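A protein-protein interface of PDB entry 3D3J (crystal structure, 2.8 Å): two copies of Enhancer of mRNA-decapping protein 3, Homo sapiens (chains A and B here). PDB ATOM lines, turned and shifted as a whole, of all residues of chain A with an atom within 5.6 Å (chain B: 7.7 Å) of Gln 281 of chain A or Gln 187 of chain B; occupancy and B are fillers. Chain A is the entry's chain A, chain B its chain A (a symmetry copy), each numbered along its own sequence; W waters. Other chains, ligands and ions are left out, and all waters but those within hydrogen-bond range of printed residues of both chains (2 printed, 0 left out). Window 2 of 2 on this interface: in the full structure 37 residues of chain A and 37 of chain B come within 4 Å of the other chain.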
ATOM      1  N   ILE A 279     -29.655  10.364  -2.952  1.00  0.00           N
ATOM      2  CA  ILE A 279     -28.538   9.465  -3.189  1.00  0.00           C
ATOM      3  C   ILE A 279     -28.625   8.936  -4.620  1.00  0.00           C
ATOM      4  O   ILE A 279     -29.623   8.311  -4.993  1.00  0.00           O
ATOM      5  CB  ILE A 279     -28.513   8.299  -2.192  1.00  0.00           C
ATOM      6  CG1 ILE A 279     -28.570   8.835  -0.760  1.00  0.00           C
ATOM      7  CG2 ILE A 279     -27.257   7.444  -2.403  1.00  0.00           C
ATOM      8  CD1 ILE A 279     -28.851   7.782   0.277  1.00  0.00           C
ATOM      9  N   PRO A 280     -27.587   9.211  -5.433  1.00  0.00           N
ATOM     10  CA  PRO A 280     -27.550   8.732  -6.810  1.00  0.00           C
ATOM     11  C   PRO A 280     -27.440   7.217  -6.872  1.00  0.00           C
ATOM     12  O   PRO A 280     -26.821   6.600  -6.003  1.00  0.00           O
ATOM     13  CB  PRO A 280     -26.280   9.381  -7.376  1.00  0.00           C
ATOM     14  CG  PRO A 280     -25.963  10.507  -6.455  1.00  0.00           C
ATOM     15  CD  PRO A 280     -26.392  10.011  -5.113  1.00  0.00           C
ATOM     16  N   GLN A 281     -28.037   6.641  -7.910  1.00  0.00           N
ATOM     17  CA  GLN A 281     -28.128   5.198  -8.079  1.00  0.00           C
ATOM     18  C   GLN A 281     -26.783   4.459  -8.035  1.00  0.00           C
ATOM     19  O   GLN A 281     -26.713   3.327  -7.556  1.00  0.00           O
ATOM     20  CB  GLN A 281     -28.848   4.882  -9.387  1.00  0.00           C
ATOM     21  CG  GLN A 281     -29.535   3.531  -9.398  1.00  0.00           C
ATOM     22  CD  GLN A 281     -29.537   2.883 -10.770  1.00  0.00           C
ATOM     23  OE1 GLN A 281     -28.521   2.884 -11.474  1.00  0.00           O
ATOM     24  NE2 GLN A 281     -30.677   2.313 -11.155  1.00  0.00           N
ATOM     25  N   GLN A 282     -25.724   5.095  -8.528  1.00  0.00           N
ATOM     26  CA  GLN A 282     -24.406   4.450  -8.582  1.00  0.00           C
ATOM     27  C   GLN A 282     -23.708   4.347  -7.225  1.00  0.00           C
ATOM     28  O   GLN A 282     -22.834   3.499  -7.037  1.00  0.00           O
ATOM     29  CB  GLN A 282     -23.497   5.138  -9.603  1.00  0.00           C
ATOM     30  CG  GLN A 282     -23.793   4.731 -11.036  1.00  0.00           C
ATOM     31  CD  GLN A 282     -23.022   5.542 -12.056  1.00  0.00           C
ATOM     32  OE1 GLN A 282     -21.788   5.537 -12.073  1.00  0.00           O
ATOM     33  NE2 GLN A 282     -23.749   6.233 -12.928  1.00  0.00           N
ATOM     34  N   VAL A 283     -24.100   5.210  -6.291  1.00  0.00           N
ATOM     35  CA  VAL A 283     -23.566   5.183  -4.929  1.00  0.00           C
ATOM     36  C   VAL A 283     -23.995   3.896  -4.208  1.00  0.00           C
ATOM     37  O   VAL A 283     -23.209   3.298  -3.468  1.00  0.00           O
ATOM     38  CB  VAL A 283     -23.988   6.450  -4.135  1.00  0.00           C
ATOM     39  CG1 VAL A 283     -23.488   6.402  -2.700  1.00  0.00           C
ATOM     40  CG2 VAL A 283     -23.472   7.701  -4.821  1.00  0.00           C
ATOM     41  N   PHE A 284     -25.240   3.475  -4.444  1.00  0.00           N
ATOM     42  CA  PHE A 284     -25.772   2.229  -3.892  1.00  0.00           C
ATOM     43  C   PHE A 284     -24.994   1.021  -4.395  1.00  0.00           C
ATOM     44  O   PHE A 284     -24.653   0.128  -3.621  1.00  0.00           O
ATOM     45  CB  PHE A 284     -27.246   2.056  -4.261  1.00  0.00           C
ATOM     46  CG  PHE A 284     -28.166   3.036  -3.594  1.00  0.00           C
ATOM     47  CD1 PHE A 284     -28.623   2.812  -2.300  1.00  0.00           C
ATOM     48  CD2 PHE A 284     -28.598   4.174  -4.272  1.00  0.00           C
ATOM     49  CE1 PHE A 284     -29.482   3.714  -1.684  1.00  0.00           C
ATOM     50  CE2 PHE A 284     -29.462   5.081  -3.666  1.00  0.00           C
ATOM     51  CZ  PHE A 284     -29.905   4.852  -2.368  1.00  0.00           C
ATOM     52  N   GLN A 285     -24.723   1.004  -5.698  1.00  0.00           N
ATOM     53  CA  GLN A 285     -24.024  -0.108  -6.335  1.00  0.00           C
ATOM     54  C   GLN A 285     -22.579  -0.227  -5.857  1.00  0.00           C
ATOM     55  O   GLN A 285     -21.995  -1.308  -5.914  1.00  0.00           O
ATOM     56  CB  GLN A 285     -24.077   0.026  -7.859  1.00  0.00           C
ATOM     57  CG  GLN A 285     -25.450  -0.267  -8.459  1.00  0.00           C
ATOM     58  CD  GLN A 285     -25.715   0.507  -9.748  1.00  0.00           C
ATOM     59  OE1 GLN A 285     -24.880   0.545 -10.660  1.00  0.00           O
ATOM     60  NE2 GLN A 285     -26.892   1.122  -9.829  1.00  0.00           N
ATOM     61  N   ILE A 289     -25.320  -2.544  -3.364  1.00  0.00           N
ATOM     62  CA  ILE A 289     -26.786  -2.523  -3.399  1.00  0.00           C
ATOM     63  C   ILE A 289     -27.308  -2.244  -4.806  1.00  0.00           C
ATOM     64  O   ILE A 289     -27.146  -1.140  -5.334  1.00  0.00           O
ATOM     65  CB  ILE A 289     -27.383  -1.459  -2.438  1.00  0.00           C
ATOM     66  CG1 ILE A 289     -26.844  -1.641  -1.016  1.00  0.00           C
ATOM     67  CG2 ILE A 289     -28.920  -1.505  -2.460  1.00  0.00           C
ATOM     68  CD1 ILE A 289     -27.047  -0.427  -0.127  1.00  0.00           C
ATOM     69  N   TYR A 291     -29.969  -0.994  -6.697  1.00  0.00           N
ATOM     70  CA  TYR A 291     -31.042  -0.073  -6.314  1.00  0.00           C
ATOM     71  C   TYR A 291     -31.871   0.429  -7.497  1.00  0.00           C
ATOM     72  O   TYR A 291     -31.327   0.810  -8.536  1.00  0.00           O
ATOM     73  CB  TYR A 291     -30.461   1.115  -5.534  1.00  0.00           C
ATOM     74  CG  TYR A 291     -31.426   2.256  -5.259  1.00  0.00           C
ATOM     75  CD1 TYR A 291     -32.293   2.218  -4.167  1.00  0.00           C
ATOM     76  CD2 TYR A 291     -31.458   3.384  -6.086  1.00  0.00           C
ATOM     77  CE1 TYR A 291     -33.174   3.273  -3.911  1.00  0.00           C
ATOM     78  CE2 TYR A 291     -32.334   4.439  -5.840  1.00  0.00           C
ATOM     79  CZ  TYR A 291     -33.188   4.379  -4.753  1.00  0.00           C
ATOM     80  OH  TYR A 291     -34.054   5.425  -4.509  1.00  0.00           O
ATOM     81  N   HIS A 292     -33.190   0.420  -7.327  1.00  0.00           N
ATOM     82  CA  HIS A 292     -34.098   1.077  -8.262  1.00  0.00           C
ATOM     83  C   HIS A 292     -35.120   1.885  -7.463  1.00  0.00           C
ATOM     84  O   HIS A 292     -35.810   1.340  -6.596  1.00  0.00           O
ATOM     85  CB  HIS A 292     -34.762   0.062  -9.202  1.00  0.00           C
ATOM     86  CG  HIS A 292     -33.815  -0.556 -10.191  1.00  0.00           C
ATOM     87  ND1 HIS A 292     -33.369  -1.857 -10.087  1.00  0.00           N
ATOM     88  CD2 HIS A 292     -33.223  -0.046 -11.300  1.00  0.00           C
ATOM     89  CE1 HIS A 292     -32.550  -2.124 -11.089  1.00  0.00           C
ATOM     90  NE2 HIS A 292     -32.443  -1.041 -11.839  1.00  0.00           N
ATOM     91  N   ARG B 153     -30.367  16.300 -11.898  1.00  0.00           N
ATOM     92  CA  ARG B 153     -29.925  15.202 -11.036  1.00  0.00           C
ATOM     93  C   ARG B 153     -31.083  14.622 -10.219  1.00  0.00           C
ATOM     94  O   ARG B 153     -31.239  13.406 -10.125  1.00  0.00           O
ATOM     95  CB  ARG B 153     -28.787  15.669 -10.123  1.00  0.00           C
ATOM     96  CG  ARG B 153     -28.469  14.720  -8.987  1.00  0.00           C
ATOM     97  CD  ARG B 153     -27.212  15.128  -8.248  1.00  0.00           C
ATOM     98  NE  ARG B 153     -27.305  16.446  -7.615  1.00  0.00           N
ATOM     99  CZ  ARG B 153     -27.742  16.666  -6.377  1.00  0.00           C
ATOM    100  NH1 ARG B 153     -28.150  15.659  -5.611  1.00  0.00           N
ATOM    101  NH2 ARG B 153     -27.778  17.904  -5.903  1.00  0.00           N
ATOM    102  N   HIS B 154     -31.900  15.499  -9.649  1.00  0.00           N
ATOM    103  CA  HIS B 154     -33.034  15.064  -8.838  1.00  0.00           C
ATOM    104  C   HIS B 154     -34.077  14.322  -9.652  1.00  0.00           C
ATOM    105  O   HIS B 154     -34.625  13.319  -9.202  1.00  0.00           O
ATOM    106  CB  HIS B 154     -33.644  16.242  -8.089  1.00  0.00           C
ATOM    107  CG  HIS B 154     -32.829  16.677  -6.912  1.00  0.00           C
ATOM    108  ND1 HIS B 154     -32.669  15.888  -5.790  1.00  0.00           N
ATOM    109  CD2 HIS B 154     -32.113  17.804  -6.688  1.00  0.00           C
ATOM    110  CE1 HIS B 154     -31.897  16.518  -4.923  1.00  0.00           C
ATOM    111  NE2 HIS B 154     -31.547  17.681  -5.442  1.00  0.00           N
ATOM    112  N   LEU B 155     -34.331  14.806 -10.864  1.00  0.00           N
ATOM    113  CA  LEU B 155     -35.237  14.122 -11.771  1.00  0.00           C
ATOM    114  C   LEU B 155     -34.707  12.728 -12.161  1.00  0.00           C
ATOM    115  O   LEU B 155     -35.453  11.746 -12.131  1.00  0.00           O
ATOM    116  CB  LEU B 155     -35.516  14.992 -13.001  1.00  0.00           C
ATOM    117  CG  LEU B 155     -36.228  16.333 -12.776  1.00  0.00           C
ATOM    118  CD1 LEU B 155     -36.045  17.221 -13.992  1.00  0.00           C
ATOM    119  CD2 LEU B 155     -37.715  16.165 -12.452  1.00  0.00           C
ATOM    120  N   ALA B 156     -33.418  12.647 -12.490  1.00  0.00           N
ATOM    121  CA  ALA B 156     -32.792  11.377 -12.854  1.00  0.00           C
ATOM    122  C   ALA B 156     -32.906  10.351 -11.730  1.00  0.00           C
ATOM    123  O   ALA B 156     -33.044   9.151 -11.989  1.00  0.00           O
ATOM    124  CB  ALA B 156     -31.337  11.585 -13.247  1.00  0.00           C
ATOM    125  N   ASN B 157     -32.850  10.837 -10.488  1.00  0.00           N
ATOM    126  CA  ASN B 157     -33.076  10.010  -9.299  1.00  0.00           C
ATOM    127  C   ASN B 157     -34.452   9.351  -9.321  1.00  0.00           C
ATOM    128  O   ASN B 157     -34.604   8.206  -8.887  1.00  0.00           O
ATOM    129  CB  ASN B 157     -32.957  10.850  -8.023  1.00  0.00           C
ATOM    130  CG  ASN B 157     -31.527  11.073  -7.588  1.00  0.00           C
ATOM    131  OD1 ASN B 157     -30.608  10.367  -8.018  1.00  0.00           O
ATOM    132  ND2 ASN B 157     -31.328  12.051  -6.712  1.00  0.00           N
ATOM    133  N   HIS B 158     -35.438  10.086  -9.837  1.00  0.00           N
ATOM    134  CA  HIS B 158     -36.835   9.669  -9.811  1.00  0.00           C
ATOM    135  C   HIS B 158     -37.280   8.971 -11.091  1.00  0.00           C
ATOM    136  O   HIS B 158     -38.440   9.087 -11.506  1.00  0.00           O
ATOM    137  CB  HIS B 158     -37.729  10.866  -9.491  1.00  0.00           C
ATOM    138  CG  HIS B 158     -37.688  11.266  -8.054  1.00  0.00           C
ATOM    139  ND1 HIS B 158     -38.537  10.731  -7.108  1.00  0.00           N
ATOM    140  CD2 HIS B 158     -36.878  12.122  -7.389  1.00  0.00           C
ATOM    141  CE1 HIS B 158     -38.261  11.252  -5.926  1.00  0.00           C
ATOM    142  NE2 HIS B 158     -37.257  12.097  -6.068  1.00  0.00           N
ATOM    143  N   ASP B 159     -36.350   8.232 -11.693  1.00  0.00           N
ATOM    144  CA  ASP B 159     -36.594   7.437 -12.898  1.00  0.00           C
ATOM    145  C   ASP B 159     -37.106   8.251 -14.095  1.00  0.00           C
ATOM    146  O   ASP B 159     -37.937   7.775 -14.869  1.00  0.00           O
ATOM    147  CB  ASP B 159     -37.517   6.244 -12.597  1.00  0.00           C
ATOM    148  CG  ASP B 159     -36.783   5.087 -11.936  1.00  0.00           C
ATOM    149  OD1 ASP B 159     -35.643   4.778 -12.348  1.00  0.00           O
ATOM    150  OD2 ASP B 159     -37.350   4.475 -11.007  1.00  0.00           O
ATOM    151  N   VAL B 160     -36.608   9.477 -14.237  1.00  0.00           N
ATOM    152  CA  VAL B 160     -36.863  10.265 -15.435  1.00  0.00           C
ATOM    153  C   VAL B 160     -35.624  10.231 -16.321  1.00  0.00           C
ATOM    154  O   VAL B 160     -34.497  10.336 -15.826  1.00  0.00           O
ATOM    155  CB  VAL B 160     -37.244  11.721 -15.103  1.00  0.00           C
ATOM    156  CG1 VAL B 160     -37.423  12.541 -16.371  1.00  0.00           C
ATOM    157  CG2 VAL B 160     -38.517  11.757 -14.284  1.00  0.00           C
ATOM    158  N   GLN B 161     -35.839  10.064 -17.624  1.00  0.00           N
ATOM    159  CA  GLN B 161     -34.754  10.084 -18.599  1.00  0.00           C
ATOM    160  C   GLN B 161     -34.247  11.508 -18.825  1.00  0.00           C
ATOM    161  O   GLN B 161     -34.831  12.291 -19.591  1.00  0.00           O
ATOM    162  CB  GLN B 161     -35.193   9.437 -19.909  1.00  0.00           C
ATOM    163  CG  GLN B 161     -35.552   7.972 -19.764  1.00  0.00           C
ATOM    164  CD  GLN B 161     -35.460   7.217 -21.072  1.00  0.00           C
ATOM    165  OE1 GLN B 161     -34.518   7.399 -21.843  1.00  0.00           O
ATOM    166  NE2 GLN B 161     -36.441   6.358 -21.329  1.00  0.00           N
ATOM    167  N   VAL B 162     -33.162  11.834 -18.128  1.00  0.00           N
ATOM    168  CA  VAL B 162     -32.566  13.158 -18.187  1.00  0.00           C
ATOM    169  C   VAL B 162     -31.399  13.145 -19.154  1.00  0.00           C
ATOM    170  O   VAL B 162     -30.449  12.370 -19.004  1.00  0.00           O
ATOM    171  CB  VAL B 162     -32.094  13.645 -16.790  1.00  0.00           C
ATOM    172  CG1 VAL B 162     -31.382  14.993 -16.889  1.00  0.00           C
ATOM    173  CG2 VAL B 162     -33.276  13.747 -15.837  1.00  0.00           C
ATOM    174  N   ILE B 163     -31.493  13.998 -20.165  1.00  0.00           N
ATOM    175  CA  ILE B 163     -30.366  14.252 -21.043  1.00  0.00           C
ATOM    176  C   ILE B 163     -30.014  15.727 -20.900  1.00  0.00           C
ATOM    177  O   ILE B 163     -30.839  16.602 -21.160  1.00  0.00           O
ATOM    178  CB  ILE B 163     -30.646  13.851 -22.517  1.00  0.00           C
ATOM    179  CG1 ILE B 163     -30.901  12.341 -22.640  1.00  0.00           C
ATOM    180  CG2 ILE B 163     -29.467  14.217 -23.399  1.00  0.00           C
ATOM    181  CD1 ILE B 163     -32.360  11.924 -22.483  1.00  0.00           C
ATOM    182  N   LEU B 182     -21.925  15.254  -9.109  1.00  0.00           N
ATOM    183  CA  LEU B 182     -23.088  14.599  -8.524  1.00  0.00           C
ATOM    184  C   LEU B 182     -23.987  14.004  -9.597  1.00  0.00           C
ATOM    185  O   LEU B 182     -24.544  12.919  -9.415  1.00  0.00           O
ATOM    186  CB  LEU B 182     -23.880  15.581  -7.658  1.00  0.00           C
ATOM    187  CG  LEU B 182     -23.361  15.854  -6.243  1.00  0.00           C
ATOM    188  CD1 LEU B 182     -23.962  17.134  -5.697  1.00  0.00           C
ATOM    189  CD2 LEU B 182     -23.650  14.685  -5.314  1.00  0.00           C
ATOM    190  N   PHE B 183     -24.123  14.719 -10.710  1.00  0.00           N
ATOM    191  CA  PHE B 183     -24.920  14.251 -11.836  1.00  0.00           C
ATOM    192  C   PHE B 183     -24.338  12.959 -12.403  1.00  0.00           C
ATOM    193  O   PHE B 183     -25.080  12.047 -12.766  1.00  0.00           O
ATOM    194  CB  PHE B 183     -24.994  15.327 -12.923  1.00  0.00           C
ATOM    195  CG  PHE B 183     -25.980  15.022 -14.020  1.00  0.00           C
ATOM    196  CD1 PHE B 183     -27.288  15.490 -13.948  1.00  0.00           C
ATOM    197  CD2 PHE B 183     -25.599  14.275 -15.135  1.00  0.00           C
ATOM    198  CE1 PHE B 183     -28.204  15.211 -14.962  1.00  0.00           C
ATOM    199  CE2 PHE B 183     -26.511  13.994 -16.153  1.00  0.00           C
ATOM    200  CZ  PHE B 183     -27.814  14.462 -16.065  1.00  0.00           C
ATOM    201  N   SER B 184     -23.009  12.892 -12.460  1.00  0.00           N
ATOM    202  CA  SER B 184     -22.287  11.726 -12.969  1.00  0.00           C
ATOM    203  C   SER B 184     -22.808  10.422 -12.383  1.00  0.00           C
ATOM    204  O   SER B 184     -22.960   9.433 -13.102  1.00  0.00           O
ATOM    205  CB  SER B 184     -20.794  11.841 -12.648  1.00  0.00           C
ATOM    206  OG  SER B 184     -20.319  13.160 -12.850  1.00  0.00           O
ATOM    207  N   LYS B 185     -23.090  10.438 -11.081  1.00  0.00           N
ATOM    208  CA  LYS B 185     -23.452   9.237 -10.321  1.00  0.00           C
ATOM    209  C   LYS B 185     -24.886   8.773 -10.569  1.00  0.00           C
ATOM    210  O   LYS B 185     -25.267   7.680 -10.143  1.00  0.00           O
ATOM    211  CB  LYS B 185     -23.224   9.456  -8.819  1.00  0.00           C
ATOM    212  CG  LYS B 185     -21.962  10.230  -8.464  1.00  0.00           C
ATOM    213  CD  LYS B 185     -20.704   9.478  -8.853  1.00  0.00           C
ATOM    214  CE  LYS B 185     -19.558  10.441  -9.052  1.00  0.00           C
ATOM    215  NZ  LYS B 185     -18.447   9.816  -9.810  1.00  0.00           N
ATOM    216  N   THR B 186     -25.674   9.601 -11.249  1.00  0.00           N
ATOM    217  CA  THR B 186     -27.023   9.214 -11.654  1.00  0.00           C
ATOM    218  C   THR B 186     -26.992   8.528 -13.017  1.00  0.00           C
ATOM    219  O   THR B 186     -25.949   8.473 -13.671  1.00  0.00           O
ATOM    220  CB  THR B 186     -27.978  10.426 -11.731  1.00  0.00           C
ATOM    221  OG1 THR B 186     -27.529  11.324 -12.753  1.00  0.00           O
ATOM    222  CG2 THR B 186     -28.051  11.162 -10.396  1.00  0.00           C
ATOM    223  N   GLN B 187     -28.144   8.010 -13.439  1.00  0.00           N
ATOM    224  CA  GLN B 187     -28.294   7.402 -14.764  1.00  0.00           C
ATOM    225  C   GLN B 187     -28.647   8.438 -15.840  1.00  0.00           C
ATOM    226  O   GLN B 187     -28.854   8.090 -17.009  1.00  0.00           O
ATOM    227  CB  GLN B 187     -29.326   6.261 -14.744  1.00  0.00           C
ATOM    228  CG  GLN B 187     -30.724   6.642 -14.247  1.00  0.00           C
ATOM    229  CD  GLN B 187     -30.853   6.556 -12.732  1.00  0.00           C
ATOM    230  OE1 GLN B 187     -30.501   7.493 -12.005  1.00  0.00           O
ATOM    231  NE2 GLN B 187     -31.369   5.428 -12.248  1.00  0.00           N
ATOM    232  N   GLY B 188     -28.717   9.708 -15.438  1.00  0.00           N
ATOM    233  CA  GLY B 188     -28.913  10.816 -16.372  1.00  0.00           C
ATOM    234  C   GLY B 188     -27.751  10.932 -17.342  1.00  0.00           C
ATOM    235  O   GLY B 188     -26.612  10.616 -17.000  1.00  0.00           O
ATOM    236  N   GLN B 189     -28.040  11.386 -18.553  1.00  0.00           N
ATOM    237  CA  GLN B 189     -27.041  11.434 -19.611  1.00  0.00           C
ATOM    238  C   GLN B 189     -26.585  12.864 -19.902  1.00  0.00           C
ATOM    239  O   GLN B 189     -27.405  13.764 -20.058  1.00  0.00           O
ATOM    240  CB  GLN B 189     -27.596  10.789 -20.876  1.00  0.00           C
ATOM    241  CG  GLN B 189     -26.526  10.348 -21.855  1.00  0.00           C
ATOM    242  CD  GLN B 189     -27.068  10.133 -23.256  1.00  0.00           C
ATOM    243  OE1 GLN B 189     -28.199  10.525 -23.570  1.00  0.00           O
ATOM    244  NE2 GLN B 189     -26.256   9.516 -24.111  1.00  0.00           N
ATOM    245  N   GLN B 190     -25.272  13.055 -19.979  1.00  0.00           N
ATOM    246  CA  GLN B 190     -24.701  14.367 -20.262  1.00  0.00           C
ATOM    247  C   GLN B 190     -24.125  14.435 -21.670  1.00  0.00           C
ATOM    248  O   GLN B 190     -23.324  13.584 -22.072  1.00  0.00           O
ATOM    249  CB  GLN B 190     -23.617  14.712 -19.243  1.00  0.00           C
ATOM    250  CG  GLN B 190     -22.870  16.001 -19.549  1.00  0.00           C
ATOM    251  CD  GLN B 190     -21.847  16.352 -18.496  1.00  0.00           C
ATOM    252  OE1 GLN B 190     -21.708  15.662 -17.484  1.00  0.00           O
ATOM    253  NE2 GLN B 190     -21.128  17.441 -18.721  1.00  0.00           N
HETATM  254  O   HOH W   1     -29.649   8.403  -9.500  1.00  0.00           O
HETATM  255  O   HOH W   2     -26.694   5.182 -12.013  1.00  0.00           O
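Among the printed residues, merely in contact across the chains: Ile 279 of chain A with Asn 157 of chain B, Pro 280 of chain A with Asn 157 of chain B, Pro 280 of chain A with Lys 185 of chain B, Pro 280 of chain A with Thr 186 of chain B and Gln 281 of chain A with Lys 185 of chain B.
No position is printed for both chains.
Of the 9 pairs that touch across the chains among the printed residues, none has its exchanged pair printed and touching as well.
The backbone NH of Gln 282 of chain A sits at hydrogen-bond distance from the backbone carbonyl oxygen of Lys 185 of chain B, at 3.1 Å.
The side-chain amide nitrogen (NE2) of Gln 282 of chain A is in hydrogen-bond range of the backbone carbonyl oxygen (O) of Ser 184 of chain B (3.3 Å).
The side-chain amide nitrogen of Gln 282 of chain A lies within hydrogen-bond range of the backbone carbonyl oxygen of Thr 186 of chain B (3.2 Å).
The side-chain amide nitrogen of Gln 281 of chain A lies close to the side-chain amide nitrogen of Gln 187 of chain B (3.4 Å).
Of the 20 printed residues of chain B, 5 touch a printed residue of chain A.
Of the 10 printed residues of chain A, 4 touch a printed residue of chain B.
Hydrophobic or aromatic side chains of chain A within 4 Å of the printed part of chain B: Pro 280.
Among the printed residues, 9 pairs touch across the chains.
The side-chain hydroxyl (OG1) of Thr 186 of chain B lies close to the backbone NH (N) of Gly 188 of chain B (3.4 Å).
The side-chain amide nitrogen of Gln 285 of chain A is in hydrogen-bond range of the side-chain amide oxygen of Gln 281 of chain A, at 2.9 Å.
The side-chain amide nitrogen of Gln 281 of chain A lies within hydrogen-bond range of the backbone carbonyl oxygen of Tyr 291 of chain A (3.1 Å).
The backbone carbonyl oxygen of Phe 183 of chain B sits at hydrogen-bond distance from the side-chain hydroxyl of Thr 186 of chain B, at 2.6 Å.
The backbone carbonyl oxygen of Ala 156 of chain B sits close to the side-chain amide oxygen of Gln 187 of chain B, 3.0 Å away.
Water W1 lies within hydrogen-bond range of OD1 of Asn 157 of chain B (2.6 Å), OE1 of Gln 187 of chain B (2.8 Å) and N of Gln 281 of chain A (2.9 Å).
Water W2 lies within hydrogen-bond range of the side-chain amide oxygen (OE1) of Gln 281 of chain A, the side-chain amide nitrogen (NE2) of Gln 282 of chain A, the backbone carbonyl oxygen (O) of Lys 185 of chain B and the backbone NH (N) of Gln 187 of chain B.
Gln 281 of chain A touches just these residues of chain B: Lys 185 and Gln 187.
Gln 187 of chain B touches just one residue of chain A: Gln 281.
Of the printed residues of chain A, Thr 186 of chain B touches Pro 280 and Gln 282.
Printed residues of chain B within 4 Å of Ile 279 of chain A: Asn 157.
Printed residues of chain A within 4 Å of Ser 184 of chain B: Gln 282.
Phe 284 of chain A touches none of the printed residues of chain B.
The nearest residue of chain A that does not touch Gln 187 of chain B is Gln 282 of chain A (4.8 Å).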
